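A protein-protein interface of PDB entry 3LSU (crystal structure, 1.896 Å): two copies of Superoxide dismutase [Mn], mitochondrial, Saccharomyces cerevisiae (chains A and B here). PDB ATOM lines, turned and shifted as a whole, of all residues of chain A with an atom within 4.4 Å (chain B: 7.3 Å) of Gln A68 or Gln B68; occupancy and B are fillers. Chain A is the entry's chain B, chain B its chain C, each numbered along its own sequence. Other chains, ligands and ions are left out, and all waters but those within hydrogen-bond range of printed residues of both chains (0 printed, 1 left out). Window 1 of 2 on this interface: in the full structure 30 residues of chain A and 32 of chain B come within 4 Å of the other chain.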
ATOM      1  N   MET A  64      19.943  -3.303 -24.294  1.00  0.00           N
ATOM      2  CA  MET A  64      20.457  -2.200 -25.102  1.00  0.00           C
ATOM      3  C   MET A  64      21.920  -2.365 -25.487  1.00  0.00           C
ATOM      4  O   MET A  64      22.324  -1.992 -26.594  1.00  0.00           O
ATOM      5  CB  MET A  64      20.262  -0.892 -24.345  1.00  0.00           C
ATOM      6  CG  MET A  64      18.811  -0.580 -24.136  1.00  0.00           C
ATOM      7  SD  MET A  64      18.578   0.743 -22.955  1.00  0.00           S
ATOM      8  CE  MET A  64      19.190   2.143 -23.886  1.00  0.00           C
ATOM      9  N   ILE A  65      22.714  -2.914 -24.570  1.00  0.00           N
ATOM     10  CA  ILE A  65      24.111  -3.233 -24.857  1.00  0.00           C
ATOM     11  C   ILE A  65      24.203  -4.214 -26.020  1.00  0.00           C
ATOM     12  O   ILE A  65      25.047  -4.069 -26.892  1.00  0.00           O
ATOM     13  CB  ILE A  65      24.821  -3.828 -23.622  1.00  0.00           C
ATOM     14  CG1 ILE A  65      24.784  -2.840 -22.461  1.00  0.00           C
ATOM     15  CG2 ILE A  65      26.266  -4.181 -23.938  1.00  0.00           C
ATOM     16  CD1 ILE A  65      25.493  -3.346 -21.219  1.00  0.00           C
ATOM     17  N   ALA A  66      23.330  -5.216 -26.034  1.00  0.00           N
ATOM     18  CA  ALA A  66      23.298  -6.173 -27.137  1.00  0.00           C
ATOM     19  C   ALA A  66      23.061  -5.478 -28.476  1.00  0.00           C
ATOM     20  O   ALA A  66      23.716  -5.789 -29.474  1.00  0.00           O
ATOM     21  CB  ALA A  66      22.224  -7.229 -26.889  1.00  0.00           C
ATOM     22  N   ILE A  67      22.134  -4.524 -28.494  1.00  0.00           N
ATOM     23  CA  ILE A  67      21.734  -3.867 -29.741  1.00  0.00           C
ATOM     24  C   ILE A  67      22.769  -2.857 -30.249  1.00  0.00           C
ATOM     25  O   ILE A  67      22.873  -2.616 -31.449  1.00  0.00           O
ATOM     26  CB  ILE A  67      20.356  -3.173 -29.599  1.00  0.00           C
ATOM     27  CG1 ILE A  67      19.267  -4.201 -29.296  1.00  0.00           C
ATOM     28  CG2 ILE A  67      19.976  -2.433 -30.880  1.00  0.00           C
ATOM     29  CD1 ILE A  67      19.174  -5.301 -30.332  1.00  0.00           C
ATOM     30  N   GLN A  68      23.543  -2.259 -29.355  1.00  0.00           N
ATOM     31  CA  GLN A  68      24.505  -1.270 -29.823  1.00  0.00           C
ATOM     32  C   GLN A  68      25.540  -1.881 -30.763  1.00  0.00           C
ATOM     33  O   GLN A  68      26.070  -1.194 -31.639  1.00  0.00           O
ATOM     34  CB  GLN A  68      25.148  -0.476 -28.672  1.00  0.00           C
ATOM     35  CG  GLN A  68      25.932  -1.280 -27.689  1.00  0.00           C
ATOM     36  CD  GLN A  68      27.256  -1.787 -28.236  1.00  0.00           C
ATOM     37  OE1 GLN A  68      27.967  -1.091 -28.978  1.00  0.00           O
ATOM     38  NE2 GLN A  68      27.605  -3.002 -27.848  1.00  0.00           N
ATOM     39  N   GLN A  69      25.824  -3.169 -30.590  1.00  0.00           N
ATOM     40  CA  GLN A  69      26.728  -3.865 -31.505  1.00  0.00           C
ATOM     41  C   GLN A  69      26.239  -3.776 -32.955  1.00  0.00           C
ATOM     42  O   GLN A  69      27.026  -3.537 -33.882  1.00  0.00           O
ATOM     43  CB  GLN A  69      26.863  -5.334 -31.101  1.00  0.00           C
ATOM     44  CG  GLN A  69      27.838  -6.109 -31.971  1.00  0.00           C
ATOM     45  CD  GLN A  69      28.074  -7.516 -31.455  1.00  0.00           C
ATOM     46  OE1 GLN A  69      27.940  -7.777 -30.252  1.00  0.00           O
ATOM     47  NE2 GLN A  69      28.424  -8.435 -32.359  1.00  0.00           N
ATOM     48  N   ASN A  70      24.936  -3.989 -33.147  1.00  0.00           N
ATOM     49  CA  ASN A  70      24.324  -3.906 -34.472  1.00  0.00           C
ATOM     50  C   ASN A  70      24.231  -2.468 -34.993  1.00  0.00           C
ATOM     51  O   ASN A  70      24.310  -2.225 -36.200  1.00  0.00           O
ATOM     52  CB  ASN A  70      22.936  -4.545 -34.455  1.00  0.00           C
ATOM     53  CG  ASN A  70      22.980  -6.032 -34.131  1.00  0.00           C
ATOM     54  OD1 ASN A  70      24.005  -6.684 -34.311  1.00  0.00           O
ATOM     55  ND2 ASN A  70      21.859  -6.573 -33.659  1.00  0.00           N
ATOM     56  N   ILE A  71      24.033  -1.513 -34.094  1.00  0.00           N
ATOM     57  CA  ILE A  71      24.044  -0.112 -34.513  1.00  0.00           C
ATOM     58  C   ILE A  71      25.428   0.238 -35.055  1.00  0.00           C
ATOM     59  O   ILE A  71      25.570   0.829 -36.136  1.00  0.00           O
ATOM     60  CB  ILE A  71      23.684   0.839 -33.360  1.00  0.00           C
ATOM     61  CG1 ILE A  71      22.197   0.679 -32.991  1.00  0.00           C
ATOM     62  CG2 ILE A  71      24.016   2.288 -33.738  1.00  0.00           C
ATOM     63  CD1 ILE A  71      21.775   1.459 -31.757  1.00  0.00           C
ATOM     64  N   MLY A  72      26.455  -0.152 -34.311  1.00  0.00           N
ATOM     65  CA  MLY A  72      27.813   0.151 -34.718  1.00  0.00           C
ATOM     66  CB  MLY A  72      28.863  -0.284 -33.648  1.00  0.00           C
ATOM     67  CG  MLY A  72      30.359   0.089 -34.020  1.00  0.00           C
ATOM     68  CD  MLY A  72      31.497  -0.152 -32.949  1.00  0.00           C
ATOM     69  CE  MLY A  72      31.285   0.469 -31.581  1.00  0.00           C
ATOM     70  NZ  MLY A  72      32.429   0.523 -30.640  1.00  0.00           N
ATOM     71  CH1 MLY A  72      33.599  -0.079 -31.262  1.00  0.00           C
ATOM     72  CH2 MLY A  72      32.065  -0.204 -29.411  1.00  0.00           C
ATOM     73  C   MLY A  72      28.156  -0.496 -36.067  1.00  0.00           C
ATOM     74  O   MLY A  72      28.727   0.110 -36.916  1.00  0.00           O
ATOM     75  N   ALA B  41      24.600   9.043 -22.317  1.00  0.00           N
ATOM     76  CA  ALA B  41      24.668   8.349 -23.607  1.00  0.00           C
ATOM     77  C   ALA B  41      23.281   8.060 -24.194  1.00  0.00           C
ATOM     78  O   ALA B  41      23.072   8.155 -25.413  1.00  0.00           O
ATOM     79  CB  ALA B  41      25.459   7.061 -23.465  1.00  0.00           C
ATOM     80  N   PHE B  45      21.730   9.440 -27.658  1.00  0.00           N
ATOM     81  CA  PHE B  45      21.119   8.582 -28.663  1.00  0.00           C
ATOM     82  C   PHE B  45      19.792   9.175 -29.088  1.00  0.00           C
ATOM     83  O   PHE B  45      19.500   9.279 -30.270  1.00  0.00           O
ATOM     84  CB  PHE B  45      20.854   7.171 -28.142  1.00  0.00           C
ATOM     85  CG  PHE B  45      19.894   6.395 -29.019  1.00  0.00           C
ATOM     86  CD1 PHE B  45      20.346   5.758 -30.165  1.00  0.00           C
ATOM     87  CD2 PHE B  45      18.537   6.347 -28.722  1.00  0.00           C
ATOM     88  CE1 PHE B  45      19.466   5.066 -30.994  1.00  0.00           C
ATOM     89  CE2 PHE B  45      17.647   5.656 -29.542  1.00  0.00           C
ATOM     90  CZ  PHE B  45      18.114   5.014 -30.679  1.00  0.00           C
ATOM     91  N   LEU B  48      20.245  12.101 -31.288  1.00  0.00           N
ATOM     92  CA  LEU B  48      20.812  11.729 -32.581  1.00  0.00           C
ATOM     93  C   LEU B  48      19.850  10.891 -33.440  1.00  0.00           C
ATOM     94  O   LEU B  48      19.866  10.979 -34.670  1.00  0.00           O
ATOM     95  CB  LEU B  48      22.145  11.005 -32.385  1.00  0.00           C
ATOM     96  CG  LEU B  48      23.311  11.883 -31.929  1.00  0.00           C
ATOM     97  CD1 LEU B  48      24.543  11.031 -31.628  1.00  0.00           C
ATOM     98  CD2 LEU B  48      23.633  12.907 -33.007  1.00  0.00           C
ATOM     99  N   ALA B  61      24.793   9.493 -39.402  1.00  0.00           N
ATOM    100  CA  ALA B  61      25.039   8.090 -39.073  1.00  0.00           C
ATOM    101  C   ALA B  61      26.366   7.975 -38.327  1.00  0.00           C
ATOM    102  O   ALA B  61      26.479   7.260 -37.330  1.00  0.00           O
ATOM    103  CB  ALA B  61      25.057   7.230 -40.344  1.00  0.00           C
ATOM    104  N   MLY B  63      27.836  10.223 -36.495  1.00  0.00           N
ATOM    105  CA  MLY B  63      27.689  10.711 -35.131  1.00  0.00           C
ATOM    106  CB  MLY B  63      26.882  12.037 -35.094  1.00  0.00           C
ATOM    107  CG  MLY B  63      27.493  13.254 -35.883  1.00  0.00           C
ATOM    108  CD  MLY B  63      26.594  14.560 -35.952  1.00  0.00           C
ATOM    109  CE  MLY B  63      27.329  15.890 -35.943  1.00  0.00           C
ATOM    110  NZ  MLY B  63      26.702  17.055 -36.604  1.00  0.00           N
ATOM    111  CH1 MLY B  63      27.738  17.840 -37.257  1.00  0.00           C
ATOM    112  CH2 MLY B  63      25.733  16.600 -37.613  1.00  0.00           C
ATOM    113  C   MLY B  63      27.041   9.663 -34.199  1.00  0.00           C
ATOM    114  O   MLY B  63      27.398   9.533 -33.083  1.00  0.00           O
ATOM    115  N   MET B  64      26.045   8.960 -34.729  1.00  0.00           N
ATOM    116  CA  MET B  64      25.351   7.897 -34.008  1.00  0.00           C
ATOM    117  C   MET B  64      26.319   6.769 -33.637  1.00  0.00           C
ATOM    118  O   MET B  64      26.341   6.299 -32.499  1.00  0.00           O
ATOM    119  CB  MET B  64      24.190   7.378 -34.870  1.00  0.00           C
ATOM    120  CG  MET B  64      23.441   6.188 -34.303  1.00  0.00           C
ATOM    121  SD  MET B  64      22.610   6.569 -32.757  1.00  0.00           S
ATOM    122  CE  MET B  64      21.196   7.522 -33.355  1.00  0.00           C
ATOM    123  N   ILE B  65      27.143   6.361 -34.597  1.00  0.00           N
ATOM    124  CA  ILE B  65      28.164   5.341 -34.360  1.00  0.00           C
ATOM    125  C   ILE B  65      29.111   5.771 -33.236  1.00  0.00           C
ATOM    126  O   ILE B  65      29.458   4.979 -32.358  1.00  0.00           O
ATOM    127  CB  ILE B  65      28.993   5.094 -35.642  1.00  0.00           C
ATOM    128  CG1 ILE B  65      28.102   4.561 -36.769  1.00  0.00           C
ATOM    129  CG2 ILE B  65      30.172   4.170 -35.366  1.00  0.00           C
ATOM    130  CD1 ILE B  65      28.770   4.643 -38.153  1.00  0.00           C
ATOM    131  N   ALA B  66      29.523   7.034 -33.265  1.00  0.00           N
ATOM    132  CA  ALA B  66      30.485   7.539 -32.286  1.00  0.00           C
ATOM    133  C   ALA B  66      30.027   7.430 -30.819  1.00  0.00           C
ATOM    134  O   ALA B  66      30.859   7.327 -29.924  1.00  0.00           O
ATOM    135  CB  ALA B  66      30.893   8.985 -32.620  1.00  0.00           C
ATOM    136  N   ILE B  67      28.722   7.445 -30.560  1.00  0.00           N
ATOM    137  CA  ILE B  67      28.253   7.325 -29.172  1.00  0.00           C
ATOM    138  C   ILE B  67      28.033   5.882 -28.693  1.00  0.00           C
ATOM    139  O   ILE B  67      27.845   5.655 -27.496  1.00  0.00           O
ATOM    140  CB  ILE B  67      26.953   8.135 -28.899  1.00  0.00           C
ATOM    141  CG1 ILE B  67      25.746   7.444 -29.527  1.00  0.00           C
ATOM    142  CG2 ILE B  67      27.080   9.573 -29.405  1.00  0.00           C
ATOM    143  CD1 ILE B  67      24.410   8.030 -29.097  1.00  0.00           C
ATOM    144  N   GLN B  68      28.074   4.914 -29.606  1.00  0.00           N
ATOM    145  CA  GLN B  68      27.846   3.515 -29.244  1.00  0.00           C
ATOM    146  C   GLN B  68      28.845   3.013 -28.215  1.00  0.00           C
ATOM    147  O   GLN B  68      28.491   2.206 -27.352  1.00  0.00           O
ATOM    148  CB  GLN B  68      27.883   2.598 -30.475  1.00  0.00           C
ATOM    149  CG  GLN B  68      26.832   2.934 -31.517  1.00  0.00           C
ATOM    150  CD  GLN B  68      25.463   3.117 -30.895  1.00  0.00           C
ATOM    151  OE1 GLN B  68      24.951   2.225 -30.211  1.00  0.00           O
ATOM    152  NE2 GLN B  68      24.865   4.282 -31.117  1.00  0.00           N
ATOM    153  N   GLN B  69      30.093   3.468 -28.311  1.00  0.00           N
ATOM    154  CA  GLN B  69      31.095   3.079 -27.326  1.00  0.00           C
ATOM    155  C   GLN B  69      30.669   3.475 -25.906  1.00  0.00           C
ATOM    156  O   GLN B  69      30.821   2.690 -24.969  1.00  0.00           O
ATOM    157  CB  GLN B  69      32.463   3.675 -27.672  1.00  0.00           C
ATOM    158  CG  GLN B  69      33.504   3.589 -26.543  1.00  0.00           C
ATOM    159  CD  GLN B  69      33.897   2.158 -26.182  1.00  0.00           C
ATOM    160  OE1 GLN B  69      33.686   1.230 -26.965  1.00  0.00           O
ATOM    161  NE2 GLN B  69      34.485   1.979 -24.991  1.00  0.00           N
ATOM    162  N   ASN B  70      30.140   4.691 -25.753  1.00  0.00           N
ATOM    163  CA  ASN B  70      29.678   5.169 -24.447  1.00  0.00           C
ATOM    164  C   ASN B  70      28.479   4.375 -23.930  1.00  0.00           C
ATOM    165  O   ASN B  70      28.413   4.016 -22.753  1.00  0.00           O
ATOM    166  CB  ASN B  70      29.359   6.664 -24.496  1.00  0.00           C
ATOM    167  CG  ASN B  70      30.611   7.523 -24.578  1.00  0.00           C
ATOM    168  OD1 ASN B  70      31.677   7.131 -24.102  1.00  0.00           O
ATOM    169  ND2 ASN B  70      30.486   8.706 -25.178  1.00  0.00           N
ATOM    170  N   ILE B  71      27.529   4.101 -24.813  1.00  0.00           N
ATOM    171  CA  ILE B  71      26.410   3.262 -24.444  1.00  0.00           C
ATOM    172  C   ILE B  71      26.903   1.914 -23.922  1.00  0.00           C
ATOM    173  O   ILE B  71      26.451   1.448 -22.879  1.00  0.00           O
ATOM    174  CB  ILE B  71      25.462   3.024 -25.624  1.00  0.00           C
ATOM    175  CG1 ILE B  71      24.696   4.313 -25.949  1.00  0.00           C
ATOM    176  CG2 ILE B  71      24.517   1.863 -25.306  1.00  0.00           C
ATOM    177  CD1 ILE B  71      23.964   4.292 -27.277  1.00  0.00           C
ATOM    178  N   MLY B  72      27.839   1.299 -24.641  1.00  0.00           N
ATOM    179  CA  MLY B  72      28.304  -0.035 -24.288  1.00  0.00           C
ATOM    180  CB  MLY B  72      29.199  -0.646 -25.406  1.00  0.00           C
ATOM    181  CG  MLY B  72      29.721  -2.122 -25.205  1.00  0.00           C
ATOM    182  CD  MLY B  72      31.002  -2.517 -26.048  1.00  0.00           C
ATOM    183  CE  MLY B  72      31.374  -3.992 -26.156  1.00  0.00           C
ATOM    184  NZ  MLY B  72      32.374  -4.363 -27.185  1.00  0.00           N
ATOM    185  CH1 MLY B  72      32.971  -5.638 -26.835  1.00  0.00           C
ATOM    186  CH2 MLY B  72      33.420  -3.327 -27.267  1.00  0.00           C
ATOM    187  C   MLY B  72      29.079  -0.027 -22.961  1.00  0.00           C
ATOM    188  O   MLY B  72      28.887  -0.850 -22.134  1.00  0.00           O
ATOM    189  N   PHE B  73      29.986   0.934 -22.828  1.00  0.00           N
ATOM    190  CA  PHE B  73      30.855   1.013 -21.654  1.00  0.00           C
ATOM    191  C   PHE B  73      30.074   1.373 -20.391  1.00  0.00           C
ATOM    192  O   PHE B  73      30.165   0.678 -19.371  1.00  0.00           O
ATOM    193  CB  PHE B  73      31.987   2.024 -21.905  1.00  0.00           C
ATOM    194  CG  PHE B  73      32.879   2.253 -20.717  1.00  0.00           C
ATOM    195  CD1 PHE B  73      33.768   1.270 -20.299  1.00  0.00           C
ATOM    196  CD2 PHE B  73      32.840   3.457 -20.025  1.00  0.00           C
ATOM    197  CE1 PHE B  73      34.597   1.477 -19.200  1.00  0.00           C
ATOM    198  CE2 PHE B  73      33.664   3.671 -18.923  1.00  0.00           C
ATOM    199  CZ  PHE B  73      34.549   2.673 -18.513  1.00  0.00           C
ATOM    200  N   HIS B  74      29.318   2.465 -20.442  1.00  0.00           N
ATOM    201  CA  HIS B  74      28.604   2.932 -19.251  1.00  0.00           C
ATOM    202  C   HIS B  74      27.398   2.052 -18.964  1.00  0.00           C
ATOM    203  O   HIS B  74      27.057   1.807 -17.802  1.00  0.00           O
ATOM    204  CB  HIS B  74      28.190   4.400 -19.387  1.00  0.00           C
ATOM    205  CG  HIS B  74      29.346   5.347 -19.377  1.00  0.00           C
ATOM    206  ND1 HIS B  74      30.117   5.559 -18.253  1.00  0.00           N
ATOM    207  CD2 HIS B  74      29.864   6.137 -20.346  1.00  0.00           C
ATOM    208  CE1 HIS B  74      31.059   6.445 -18.532  1.00  0.00           C
ATOM    209  NE2 HIS B  74      30.923   6.815 -19.794  1.00  0.00           N
ATOM    210  N   ASP B 155      32.581  -4.735 -20.657  1.00  0.00           N
ATOM    211  CA  ASP B 155      31.847  -5.682 -21.483  1.00  0.00           C
ATOM    212  C   ASP B 155      31.134  -6.616 -20.531  1.00  0.00           C
ATOM    213  O   ASP B 155      31.586  -6.831 -19.409  1.00  0.00           O
ATOM    214  CB  ASP B 155      32.786  -6.471 -22.399  1.00  0.00           C
ATOM    215  CG  ASP B 155      33.513  -5.577 -23.395  1.00  0.00           C
ATOM    216  OD1 ASP B 155      33.182  -4.372 -23.479  1.00  0.00           O
ATOM    217  OD2 ASP B 155      34.423  -6.079 -24.080  1.00  0.00           O
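The side-chain amide nitrogen (NE2) of Gln B68 is in hydrogen-bond range of the backbone carbonyl oxygen (O) of Met B64. OD1 of Asp B155 lies close to NZ of MLY B72, 3.8 Å away. O of Ile A65 is in hydrogen-bond range of NE2 of Gln A68, at 2.9 Å.
Along chain A the printed residues that touch a printed residue of chain B span positions 68 to 72. Among the printed residues, 5 pairs touch across the chains.
CB of Gln A68 touches OE1 of Gln B68, 3.1 Å away. Gln A68 touches MLY B72. Met B64 touches Ile A71 (CG to CG2, 3.98 Å). Gln B68 touches Ile A71 (CD to CG2, 3.3 Å). Gln B69 touches MLY A72.
Ala A66 touches none of the printed residues of chain B. Gln A68 touches just these residues of chain B: Gln B68 and MLY B72. Of the printed residues of chain B, Ile A71 touches Met B64 (3.98 Å) and Gln B68 (3.3 Å). Printed residues of chain B within 4 Å of MLY A72: Gln B69 (3.3 Å). Phe B45 touches none of the printed residues of chain A. Printed residues of chain A within 4 Å of Met B64: Ile A71. Gln B68 touches just these residues of chain A: Gln A68 (3.1 Å) and Ile A71 (3.3 Å). Printed residues of chain A within 4 Å of Gln B69: MLY A72. Printed residues of chain A within 4 Å of MLY B72: Gln A68. The nearest residue of chain B that does not touch Gln A68 is Ile B71 (4.1 Å).
Gln B68 touches its own counterpart, Gln A68. Ile A71 touches Met B64, but with the chains exchanged Met A64 does not touch Ile B71 (4.6 Å). Ile A71 touches Gln B68, but with the chains exchanged Gln A68 does not touch Ile B71 (4.1 Å). MLY A72 touches Gln B69, but with the chains exchanged Gln A69 does not touch MLY B72 (6.4 Å).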
